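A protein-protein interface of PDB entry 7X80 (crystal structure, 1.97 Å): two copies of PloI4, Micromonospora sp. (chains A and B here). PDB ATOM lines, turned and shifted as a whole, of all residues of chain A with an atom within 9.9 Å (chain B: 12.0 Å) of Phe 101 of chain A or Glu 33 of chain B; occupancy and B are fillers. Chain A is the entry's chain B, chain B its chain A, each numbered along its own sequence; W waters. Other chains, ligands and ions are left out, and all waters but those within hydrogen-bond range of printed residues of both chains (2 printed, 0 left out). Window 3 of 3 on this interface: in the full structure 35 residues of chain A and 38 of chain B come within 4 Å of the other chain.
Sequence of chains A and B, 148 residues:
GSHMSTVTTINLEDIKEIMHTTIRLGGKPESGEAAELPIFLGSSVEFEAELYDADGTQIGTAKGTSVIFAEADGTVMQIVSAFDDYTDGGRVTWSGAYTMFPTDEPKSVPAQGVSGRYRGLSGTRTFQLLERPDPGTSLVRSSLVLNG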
ATOM      1  N   ILE A  68       3.502  10.485 -20.616  1.00  0.00           N
ATOM      2  CA  ILE A  68       4.036  11.812 -20.302  1.00  0.00           C
ATOM      3  C   ILE A  68       3.159  12.900 -20.922  1.00  0.00           C
ATOM      4  O   ILE A  68       2.687  12.772 -22.061  1.00  0.00           O
ATOM      5  CB  ILE A  68       5.495  11.936 -20.792  1.00  0.00           C
ATOM      6  CG1 ILE A  68       6.417  10.914 -20.091  1.00  0.00           C
ATOM      7  CG2 ILE A  68       5.996  13.362 -20.617  1.00  0.00           C
ATOM      8  CD1 ILE A  68       7.876  10.949 -20.607  1.00  0.00           C
ATOM      9  N   PHE A  69       2.934  13.981 -20.173  1.00  0.00           N
ATOM     10  CA  PHE A  69       2.264  15.174 -20.699  1.00  0.00           C
ATOM     11  C   PHE A  69       2.766  16.380 -19.910  1.00  0.00           C
ATOM     12  O   PHE A  69       3.664  16.258 -19.074  1.00  0.00           O
ATOM     13  CB  PHE A  69       0.732  15.040 -20.637  1.00  0.00           C
ATOM     14  CG  PHE A  69       0.157  15.131 -19.240  1.00  0.00           C
ATOM     15  CD1 PHE A  69       0.271  14.071 -18.350  1.00  0.00           C
ATOM     16  CD2 PHE A  69      -0.529  16.276 -18.832  1.00  0.00           C
ATOM     17  CE1 PHE A  69      -0.282  14.155 -17.074  1.00  0.00           C
ATOM     18  CE2 PHE A  69      -1.078  16.372 -17.563  1.00  0.00           C
ATOM     19  CZ  PHE A  69      -0.951  15.306 -16.672  1.00  0.00           C
ATOM     20  N   ALA A  70       2.190  17.559 -20.168  1.00  0.00           N
ATOM     21  CA  ALA A  70       2.666  18.751 -19.479  1.00  0.00           C
ATOM     22  C   ALA A  70       1.513  19.672 -19.114  1.00  0.00           C
ATOM     23  O   ALA A  70       0.478  19.715 -19.783  1.00  0.00           O
ATOM     24  CB  ALA A  70       3.695  19.527 -20.308  1.00  0.00           C
ATOM     25  N   GLY A  74       4.280  24.560 -17.558  1.00  0.00           N
ATOM     26  CA  GLY A  74       5.460  23.912 -18.080  1.00  0.00           C
ATOM     27  C   GLY A  74       5.882  22.688 -17.302  1.00  0.00           C
ATOM     28  O   GLY A  74       6.870  22.044 -17.683  1.00  0.00           O
ATOM     29  N   THR A  75       5.165  22.343 -16.228  1.00  0.00           N
ATOM     30  CA  THR A  75       5.523  21.176 -15.424  1.00  0.00           C
ATOM     31  C   THR A  75       5.299  19.896 -16.225  1.00  0.00           C
ATOM     32  O   THR A  75       4.171  19.602 -16.642  1.00  0.00           O
ATOM     33  CB  THR A  75       4.699  21.132 -14.138  1.00  0.00           C
ATOM     34  OG1 THR A  75       4.787  22.390 -13.458  1.00  0.00           O
ATOM     35  CG2 THR A  75       5.211  20.027 -13.231  1.00  0.00           C
ATOM     36  N   VAL A  76       6.359  19.129 -16.422  1.00  0.00           N
ATOM     37  CA  VAL A  76       6.229  17.837 -17.081  1.00  0.00           C
ATOM     38  C   VAL A  76       5.648  16.832 -16.095  1.00  0.00           C
ATOM     39  O   VAL A  76       6.143  16.681 -14.971  1.00  0.00           O
ATOM     40  CB  VAL A  76       7.580  17.371 -17.640  1.00  0.00           C
ATOM     41  CG1 VAL A  76       7.403  16.049 -18.365  1.00  0.00           C
ATOM     42  CG2 VAL A  76       8.109  18.413 -18.592  1.00  0.00           C
ATOM     43  N   MET A  77       4.592  16.148 -16.520  1.00  0.00           N
ATOM     44  CA  MET A  77       3.770  15.307 -15.677  1.00  0.00           C
ATOM     45  C   MET A  77       3.769  13.902 -16.278  1.00  0.00           C
ATOM     46  O   MET A  77       4.113  13.706 -17.445  1.00  0.00           O
ATOM     47  CB  MET A  77       2.336  15.861 -15.638  1.00  0.00           C
ATOM     48  CG  MET A  77       2.183  17.198 -14.896  1.00  0.00           C
ATOM     49  SD  MET A  77       2.705  17.336 -13.171  1.00  0.00           S
ATOM     50  CE  MET A  77       1.467  16.317 -12.366  1.00  0.00           C
ATOM     51  N   GLN A  78       3.393  12.919 -15.477  1.00  0.00           N
ATOM     52  CA  GLN A  78       3.005  11.612 -15.980  1.00  0.00           C
ATOM     53  C   GLN A  78       1.637  11.283 -15.423  1.00  0.00           C
ATOM     54  O   GLN A  78       1.337  11.612 -14.273  1.00  0.00           O
ATOM     55  CB  GLN A  78       4.035  10.528 -15.601  1.00  0.00           C
ATOM     56  CG  GLN A  78       5.415  10.852 -16.184  1.00  0.00           C
ATOM     57  CD  GLN A  78       6.442   9.735 -16.036  1.00  0.00           C
ATOM     58  OE1 GLN A  78       6.146   8.652 -15.532  1.00  0.00           O
ATOM     59  NE2 GLN A  78       7.660   9.994 -16.512  1.00  0.00           N
ATOM     60  N   TYR A  98       1.307  12.691 -11.588  1.00  0.00           N
ATOM     61  CA  TYR A  98       2.390  13.068 -10.685  1.00  0.00           C
ATOM     62  C   TYR A  98       3.483  13.753 -11.497  1.00  0.00           C
ATOM     63  O   TYR A  98       3.589  13.566 -12.711  1.00  0.00           O
ATOM     64  CB  TYR A  98       2.961  11.849  -9.925  1.00  0.00           C
ATOM     65  CG  TYR A  98       3.430  10.750 -10.840  1.00  0.00           C
ATOM     66  CD1 TYR A  98       4.728  10.733 -11.316  1.00  0.00           C
ATOM     67  CD2 TYR A  98       2.552   9.771 -11.287  1.00  0.00           C
ATOM     68  CE1 TYR A  98       5.158   9.754 -12.176  1.00  0.00           C
ATOM     69  CE2 TYR A  98       2.972   8.781 -12.155  1.00  0.00           C
ATOM     70  CZ  TYR A  98       4.277   8.779 -12.595  1.00  0.00           C
ATOM     71  OH  TYR A  98       4.714   7.805 -13.461  1.00  0.00           O
ATOM     72  N   THR A  99       4.299  14.552 -10.816  1.00  0.00           N
ATOM     73  CA  THR A  99       5.398  15.230 -11.489  1.00  0.00           C
ATOM     74  C   THR A  99       6.449  14.228 -11.948  1.00  0.00           C
ATOM     75  O   THR A  99       6.806  13.295 -11.226  1.00  0.00           O
ATOM     76  CB  THR A  99       6.040  16.260 -10.565  1.00  0.00           C
ATOM     77  OG1 THR A  99       6.643  15.578  -9.454  1.00  0.00           O
ATOM     78  CG2 THR A  99       4.991  17.236 -10.056  1.00  0.00           C
ATOM     79  N   MET A 100       6.943  14.420 -13.167  1.00  0.00           N
ATOM     80  CA  MET A 100       7.990  13.532 -13.657  1.00  0.00           C
ATOM     81  C   MET A 100       9.309  13.782 -12.944  1.00  0.00           C
ATOM     82  O   MET A 100      10.010  12.834 -12.573  1.00  0.00           O
ATOM     83  CB  MET A 100       8.150  13.689 -15.164  1.00  0.00           C
ATOM     84  CG  MET A 100       9.253  12.787 -15.723  1.00  0.00           C
ATOM     85  SD  MET A 100       9.253  12.795 -17.509  1.00  0.00           S
ATOM     86  CE  MET A 100      10.629  11.683 -17.872  1.00  0.00           C
ATOM     87  N   PHE A 101       9.650  15.036 -12.725  1.00  0.00           N
ATOM     88  CA  PHE A 101      10.964  15.379 -12.218  1.00  0.00           C
ATOM     89  C   PHE A 101      10.884  15.872 -10.781  1.00  0.00           C
ATOM     90  O   PHE A 101       9.926  16.560 -10.416  1.00  0.00           O
ATOM     91  CB  PHE A 101      11.610  16.447 -13.111  1.00  0.00           C
ATOM     92  CG  PHE A 101      11.852  15.967 -14.504  1.00  0.00           C
ATOM     93  CD1 PHE A 101      12.888  15.088 -14.775  1.00  0.00           C
ATOM     94  CD2 PHE A 101      11.018  16.342 -15.536  1.00  0.00           C
ATOM     95  CE1 PHE A 101      13.107  14.620 -16.067  1.00  0.00           C
ATOM     96  CE2 PHE A 101      11.224  15.879 -16.819  1.00  0.00           C
ATOM     97  CZ  PHE A 101      12.272  15.019 -17.093  1.00  0.00           C
ATOM     98  N   PRO A 102      11.856  15.500  -9.930  1.00  0.00           N
ATOM     99  CA  PRO A 102      12.994  14.643 -10.297  1.00  0.00           C
ATOM    100  C   PRO A 102      12.614  13.164 -10.417  1.00  0.00           C
ATOM    101  O   PRO A 102      11.697  12.696  -9.737  1.00  0.00           O
ATOM    102  CB  PRO A 102      13.979  14.848  -9.143  1.00  0.00           C
ATOM    103  CG  PRO A 102      13.147  15.279  -7.986  1.00  0.00           C
ATOM    104  CD  PRO A 102      11.830  15.816  -8.492  1.00  0.00           C
ATOM    105  N   THR A 103      13.311  12.431 -11.280  1.00  0.00           N
ATOM    106  CA  THR A 103      12.877  11.074 -11.585  1.00  0.00           C
ATOM    107  C   THR A 103      13.178  10.082 -10.466  1.00  0.00           C
ATOM    108  O   THR A 103      12.611   8.985 -10.467  1.00  0.00           O
ATOM    109  CB  THR A 103      13.526  10.600 -12.880  1.00  0.00           C
ATOM    110  OG1 THR A 103      14.941  10.501 -12.686  1.00  0.00           O
ATOM    111  CG2 THR A 103      13.218  11.579 -14.016  1.00  0.00           C
ATOM    112  N   ASP A 104      14.036  10.433  -9.513  1.00  0.00           N
ATOM    113  CA  ASP A 104      14.461   9.488  -8.485  1.00  0.00           C
ATOM    114  C   ASP A 104      13.733   9.648  -7.153  1.00  0.00           C
ATOM    115  O   ASP A 104      14.022   8.889  -6.227  1.00  0.00           O
ATOM    116  CB  ASP A 104      15.978   9.596  -8.259  1.00  0.00           C
ATOM    117  CG  ASP A 104      16.414  10.975  -7.784  1.00  0.00           C
ATOM    118  OD1 ASP A 104      15.568  11.896  -7.651  1.00  0.00           O
ATOM    119  OD2 ASP A 104      17.618  11.132  -7.512  1.00  0.00           O
ATOM    120  N   GLU A 105      12.803  10.619  -7.022  1.00  0.00           N
ATOM    121  CA  GLU A 105      12.055  10.786  -5.777  1.00  0.00           C
ATOM    122  C   GLU A 105      10.811   9.903  -5.763  1.00  0.00           C
ATOM    123  O   GLU A 105      10.337   9.464  -6.819  1.00  0.00           O
ATOM    124  CB  GLU A 105      11.652  12.253  -5.589  1.00  0.00           C
ATOM    125  CG  GLU A 105      10.634  12.740  -6.613  1.00  0.00           C
ATOM    126  CD  GLU A 105       9.922  14.040  -6.232  1.00  0.00           C
ATOM    127  OE1 GLU A 105      10.408  14.760  -5.330  1.00  0.00           O
ATOM    128  OE2 GLU A 105       8.900  14.368  -6.890  1.00  0.00           O
ATOM    129  N   PRO A 106      10.265   9.617  -4.573  1.00  0.00           N
ATOM    130  CA  PRO A 106       9.026   8.828  -4.497  1.00  0.00           C
ATOM    131  C   PRO A 106       7.855   9.603  -5.062  1.00  0.00           C
ATOM    132  O   PRO A 106       7.738  10.815  -4.865  1.00  0.00           O
ATOM    133  CB  PRO A 106       8.835   8.581  -2.990  1.00  0.00           C
ATOM    134  CG  PRO A 106      10.144   8.958  -2.337  1.00  0.00           C
ATOM    135  CD  PRO A 106      10.752  10.002  -3.231  1.00  0.00           C
ATOM    136  N   LYS A 107       6.987   8.895  -5.773  1.00  0.00           N
ATOM    137  CA  LYS A 107       5.783   9.470  -6.352  1.00  0.00           C
ATOM    138  C   LYS A 107       4.574   8.769  -5.749  1.00  0.00           C
ATOM    139  O   LYS A 107       4.666   7.617  -5.320  1.00  0.00           O
ATOM    140  CB  LYS A 107       5.765   9.313  -7.889  1.00  0.00           C
ATOM    141  CG  LYS A 107       7.036   9.750  -8.602  1.00  0.00           C
ATOM    142  CD  LYS A 107       7.249  11.260  -8.546  1.00  0.00           C
ATOM    143  CE  LYS A 107       8.609  11.600  -9.176  1.00  0.00           C
ATOM    144  NZ  LYS A 107       8.822  13.051  -9.425  1.00  0.00           N
ATOM    145  N   LEU A 129      11.611   5.103  -8.270  1.00  0.00           N
ATOM    146  CA  LEU A 129      12.551   4.426  -9.160  1.00  0.00           C
ATOM    147  C   LEU A 129      13.936   4.341  -8.516  1.00  0.00           C
ATOM    148  O   LEU A 129      14.561   5.373  -8.251  1.00  0.00           O
ATOM    149  CB  LEU A 129      12.634   5.182 -10.487  1.00  0.00           C
ATOM    150  CG  LEU A 129      13.393   4.532 -11.635  1.00  0.00           C
ATOM    151  CD1 LEU A 129      12.994   3.074 -11.771  1.00  0.00           C
ATOM    152  CD2 LEU A 129      13.133   5.304 -12.932  1.00  0.00           C
ATOM    153  N   GLY B  27       3.754  17.913 -27.607  1.00  0.00           N
ATOM    154  CA  GLY B  27       4.855  17.923 -28.549  1.00  0.00           C
ATOM    155  C   GLY B  27       6.189  17.750 -27.844  1.00  0.00           C
ATOM    156  O   GLY B  27       6.269  17.156 -26.762  1.00  0.00           O
ATOM    157  N   LYS B  28       7.236  18.268 -28.474  1.00  0.00           N
ATOM    158  CA  LYS B  28       8.561  18.056 -27.899  1.00  0.00           C
ATOM    159  C   LYS B  28       8.821  19.094 -26.804  1.00  0.00           C
ATOM    160  O   LYS B  28       8.478  20.266 -26.967  1.00  0.00           O
ATOM    161  CB  LYS B  28       9.633  18.132 -28.997  1.00  0.00           C
ATOM    162  CG  LYS B  28      11.060  18.234 -28.489  1.00  0.00           C
ATOM    163  CD  LYS B  28      12.081  17.793 -29.553  1.00  0.00           C
ATOM    164  CE  LYS B  28      11.924  16.314 -29.945  1.00  0.00           C
ATOM    165  NZ  LYS B  28      11.973  15.346 -28.786  1.00  0.00           N
ATOM    166  N   PRO B  29       9.384  18.696 -25.661  1.00  0.00           N
ATOM    167  CA  PRO B  29       9.637  19.677 -24.599  1.00  0.00           C
ATOM    168  C   PRO B  29      10.676  20.696 -25.046  1.00  0.00           C
ATOM    169  O   PRO B  29      11.654  20.361 -25.715  1.00  0.00           O
ATOM    170  CB  PRO B  29      10.136  18.826 -23.424  1.00  0.00           C
ATOM    171  CG  PRO B  29      10.505  17.525 -24.000  1.00  0.00           C
ATOM    172  CD  PRO B  29       9.714  17.322 -25.249  1.00  0.00           C
ATOM    173  N   GLU B  30      10.439  21.958 -24.705  1.00  0.00           N
ATOM    174  CA  GLU B  30      11.272  23.015 -25.259  1.00  0.00           C
ATOM    175  C   GLU B  30      12.364  23.491 -24.312  1.00  0.00           C
ATOM    176  O   GLU B  30      13.346  24.078 -24.778  1.00  0.00           O
ATOM    177  CB  GLU B  30      10.405  24.211 -25.694  1.00  0.00           C
ATOM    178  CG  GLU B  30      10.222  25.307 -24.644  1.00  0.00           C
ATOM    179  CD  GLU B  30       9.025  25.078 -23.736  1.00  0.00           C
ATOM    180  OE1 GLU B  30       8.558  23.920 -23.634  1.00  0.00           O
ATOM    181  OE2 GLU B  30       8.552  26.062 -23.124  1.00  0.00           O
ATOM    182  N   SER B  31      12.237  23.243 -23.011  1.00  0.00           N
ATOM    183  CA  SER B  31      13.225  23.721 -22.056  1.00  0.00           C
ATOM    184  C   SER B  31      13.471  22.669 -20.983  1.00  0.00           C
ATOM    185  O   SER B  31      12.777  21.651 -20.895  1.00  0.00           O
ATOM    186  CB  SER B  31      12.784  25.041 -21.408  1.00  0.00           C
ATOM    187  OG  SER B  31      11.499  24.922 -20.820  1.00  0.00           O
ATOM    188  N   GLY B  32      14.493  22.928 -20.176  1.00  0.00           N
ATOM    189  CA  GLY B  32      14.723  22.177 -18.966  1.00  0.00           C
ATOM    190  C   GLY B  32      15.243  20.761 -19.174  1.00  0.00           C
ATOM    191  O   GLY B  32      15.772  20.385 -20.229  1.00  0.00           O
ATOM    192  N   GLU B  33      15.075  19.975 -18.108  1.00  0.00           N
ATOM    193  CA  GLU B  33      15.576  18.606 -18.075  1.00  0.00           C
ATOM    194  C   GLU B  33      14.917  17.746 -19.144  1.00  0.00           C
ATOM    195  O   GLU B  33      15.586  16.942 -19.805  1.00  0.00           O
ATOM    196  CB  GLU B  33      15.321  18.019 -16.691  1.00  0.00           C
ATOM    197  CG  GLU B  33      16.013  16.708 -16.403  1.00  0.00           C
ATOM    198  CD  GLU B  33      16.045  16.421 -14.911  1.00  0.00           C
ATOM    199  OE1 GLU B  33      16.386  15.277 -14.525  1.00  0.00           O
ATOM    200  OE2 GLU B  33      15.700  17.343 -14.129  1.00  0.00           O
ATOM    201  N   ALA B  34      13.602  17.905 -19.324  1.00  0.00           N
ATOM    202  CA  ALA B  34      12.869  17.101 -20.297  1.00  0.00           C
ATOM    203  C   ALA B  34      13.391  17.296 -21.716  1.00  0.00           C
ATOM    204  O   ALA B  34      13.346  16.358 -22.522  1.00  0.00           O
ATOM    205  CB  ALA B  34      11.380  17.441 -20.235  1.00  0.00           C
ATOM    206  N   ALA B  35      13.884  18.495 -22.041  1.00  0.00           N
ATOM    207  CA  ALA B  35      14.314  18.778 -23.409  1.00  0.00           C
ATOM    208  C   ALA B  35      15.516  17.928 -23.806  1.00  0.00           C
ATOM    209  O   ALA B  35      15.622  17.493 -24.957  1.00  0.00           O
ATOM    210  CB  ALA B  35      14.632  20.266 -23.567  1.00  0.00           C
ATOM    211  N   GLU B  36      16.425  17.673 -22.866  1.00  0.00           N
ATOM    212  CA  GLU B  36      17.570  16.803 -23.107  1.00  0.00           C
ATOM    213  C   GLU B  36      17.184  15.340 -23.283  1.00  0.00           C
ATOM    214  O   GLU B  36      18.031  14.541 -23.697  1.00  0.00           O
ATOM    215  CB  GLU B  36      18.560  16.923 -21.947  1.00  0.00           C
ATOM    216  CG  GLU B  36      19.451  18.145 -21.996  1.00  0.00           C
ATOM    217  CD  GLU B  36      20.321  18.247 -20.763  1.00  0.00           C
ATOM    218  OE1 GLU B  36      19.785  18.636 -19.702  1.00  0.00           O
ATOM    219  OE2 GLU B  36      21.526  17.922 -20.846  1.00  0.00           O
ATOM    220  N   LEU B  37      15.948  14.968 -22.974  1.00  0.00           N
ATOM    221  CA  LEU B  37      15.518  13.583 -22.990  1.00  0.00           C
ATOM    222  C   LEU B  37      14.753  13.270 -24.274  1.00  0.00           C
ATOM    223  O   LEU B  37      14.143  14.157 -24.877  1.00  0.00           O
ATOM    224  CB  LEU B  37      14.637  13.308 -21.767  1.00  0.00           C
ATOM    225  CG  LEU B  37      15.397  13.079 -20.454  1.00  0.00           C
ATOM    226  CD1 LEU B  37      14.461  12.669 -19.323  1.00  0.00           C
ATOM    227  CD2 LEU B  37      16.490  12.038 -20.644  1.00  0.00           C
ATOM    228  N   PRO B  38      14.766  12.026 -24.745  1.00  0.00           N
ATOM    229  CA  PRO B  38      13.929  11.678 -25.894  1.00  0.00           C
ATOM    230  C   PRO B  38      12.509  11.324 -25.439  1.00  0.00           C
ATOM    231  O   PRO B  38      12.135  10.174 -25.181  1.00  0.00           O
ATOM    232  CB  PRO B  38      14.690  10.496 -26.490  1.00  0.00           C
ATOM    233  CG  PRO B  38      15.150   9.732 -25.227  1.00  0.00           C
ATOM    234  CD  PRO B  38      15.166  10.776 -24.066  1.00  0.00           C
ATOM    235  N   ILE B  39      11.691  12.361 -25.281  1.00  0.00           N
ATOM    236  CA  ILE B  39      10.310  12.211 -24.847  1.00  0.00           C
ATOM    237  C   ILE B  39       9.434  13.149 -25.661  1.00  0.00           C
ATOM    238  O   ILE B  39       9.895  14.154 -26.207  1.00  0.00           O
ATOM    239  CB  ILE B  39      10.116  12.488 -23.340  1.00  0.00           C
ATOM    240  CG1 ILE B  39      10.035  13.985 -23.073  1.00  0.00           C
ATOM    241  CG2 ILE B  39      11.184  11.831 -22.488  1.00  0.00           C
ATOM    242  CD1 ILE B  39       9.663  14.305 -21.648  1.00  0.00           C
ATOM    243  N   PHE B  40       8.153  12.792 -25.746  1.00  0.00           N
ATOM    244  CA  PHE B  40       7.125  13.668 -26.290  1.00  0.00           C
ATOM    245  C   PHE B  40       6.042  13.855 -25.242  1.00  0.00           C
ATOM    246  O   PHE B  40       5.668  12.903 -24.547  1.00  0.00           O
ATOM    247  CB  PHE B  40       6.496  13.105 -27.568  1.00  0.00           C
ATOM    248  CG  PHE B  40       7.334  13.317 -28.805  1.00  0.00           C
ATOM    249  CD1 PHE B  40       8.358  12.440 -29.124  1.00  0.00           C
ATOM    250  CD2 PHE B  40       7.103  14.411 -29.636  1.00  0.00           C
ATOM    251  CE1 PHE B  40       9.129  12.638 -30.275  1.00  0.00           C
ATOM    252  CE2 PHE B  40       7.878  14.614 -30.784  1.00  0.00           C
ATOM    253  CZ  PHE B  40       8.881  13.724 -31.094  1.00  0.00           C
ATOM    254  N   LEU B  41       5.571  15.088 -25.116  1.00  0.00           N
ATOM    255  CA  LEU B  41       4.416  15.382 -24.279  1.00  0.00           C
ATOM    256  C   LEU B  41       3.170  15.036 -25.072  1.00  0.00           C
ATOM    257  O   LEU B  41       2.955  15.591 -26.157  1.00  0.00           O
ATOM    258  CB  LEU B  41       4.414  16.856 -23.886  1.00  0.00           C
ATOM    259  CG  LEU B  41       5.778  17.358 -23.375  1.00  0.00           C
ATOM    260  CD1 LEU B  41       5.777  18.878 -23.184  1.00  0.00           C
ATOM    261  CD2 LEU B  41       6.225  16.647 -22.123  1.00  0.00           C
ATOM    262  N   GLY B  42       2.370  14.099 -24.564  1.00  0.00           N
ATOM    263  CA  GLY B  42       1.123  13.777 -25.229  1.00  0.00           C
ATOM    264  C   GLY B  42       0.161  14.952 -25.211  1.00  0.00           C
ATOM    265  O   GLY B  42       0.171  15.777 -24.293  1.00  0.00           O
HETATM  266  O   HOH W   1       0.277  17.968 -22.540  1.00  0.00           O
HETATM  267  O   HOH W   2      15.707  13.705 -12.278  1.00  0.00           O
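The backbone carbonyl oxygen (O) of Ile 68 of chain A sits at hydrogen-bond distance from the backbone NH (N) of Gly 42 of chain B (2.9 Å).
O of Phe 69 of chain A lies within hydrogen-bond range of N of Met 77 of chain A, 2.7 Å away. The backbone NH (N) of Met 100 of chain A sits at hydrogen-bond distance from the backbone carbonyl oxygen (O) of Val 76 of chain A, 3.0 Å away. N of Leu 41 of chain B sits at hydrogen-bond distance from O of Gly 27 of chain B, at 2.7 Å.
Among the printed residues, pairs that only touch across the chains: Ile 68 of chain A with Ile 39 of chain B, Ile 68 of chain A with Phe 40 of chain B, Ile 68 of chain A with Leu 41 of chain B, Phe 69 of chain A with Gly 42 of chain B, Ala 70 of chain A with Leu 41 of chain B, Val 76 of chain A with Ala 34 of chain B, Val 76 of chain A with Leu 41 of chain B, Phe 101 of chain A with Glu 33 of chain B, Phe 101 of chain A with Ala 34 of chain B and Phe 101 of chain A with Leu 37 of chain B.
Printed residues of chain B within 4 Å of Ile 68 of chain A: Ile 39 (3.9 Å), Phe 40 (3.9 Å), Leu 41 (3.6 Å) and Gly 42 (2.9 Å). Of the printed residues of chain B, Phe 69 of chain A touches Gly 42 (3.8 Å). Thr 75 of chain A touches none of the printed residues of chain B. Met 77 of chain A touches none of the printed residues of chain B. No residue of chain B comes within 4 Å of Thr 99 of chain A. No residue of chain B comes within 4 Å of Met 100 of chain A. Phe 101 of chain A touches just these residues of chain B: Glu 33, Ala 34 and Leu 37. No residue of chain B comes within 4 Å of Pro 102 of chain A. Gly 32 of chain B touches none of the printed residues of chain A. Glu 33 of chain B touches just one residue of chain A: Phe 101 (3.4 Å). Printed residues of chain A within 4 Å of Ala 34 of chain B: Val 76 (3.8 Å) and Phe 101 (3.8 Å). Ala 35 of chain B touches none of the printed residues of chain A. Printed residues of chain A within 4 Å of Leu 37 of chain B: Phe 101 (3.9 Å). Of the printed residues of chain A, Leu 41 of chain B touches Ile 68, Ala 70 and Val 76. Printed residues of chain A within 4 Å of Gly 42 of chain B: Ile 68 and Phe 69. The nearest residue of chain B that does not touch Phe 101 of chain A is Ile 39 of chain B (5.3 Å). The nearest printed residue of chain A that does not touch Phe 40 of chain B is Phe 69 of chain A (5.3 Å).
Among the printed residues, 11 pairs touch across the chains.
No position is printed for both chains.
Water W1 lies within hydrogen-bond range of the backbone carbonyl oxygen of Gly 42 of chain B (2.8 Å) and the backbone NH of Ala 70 of chain A (3.1 Å). Water W2 lies within hydrogen-bond range of OE1 of Glu 33 of chain B (2.8 Å) and N of Thr 103 of chain A (2.9 Å).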
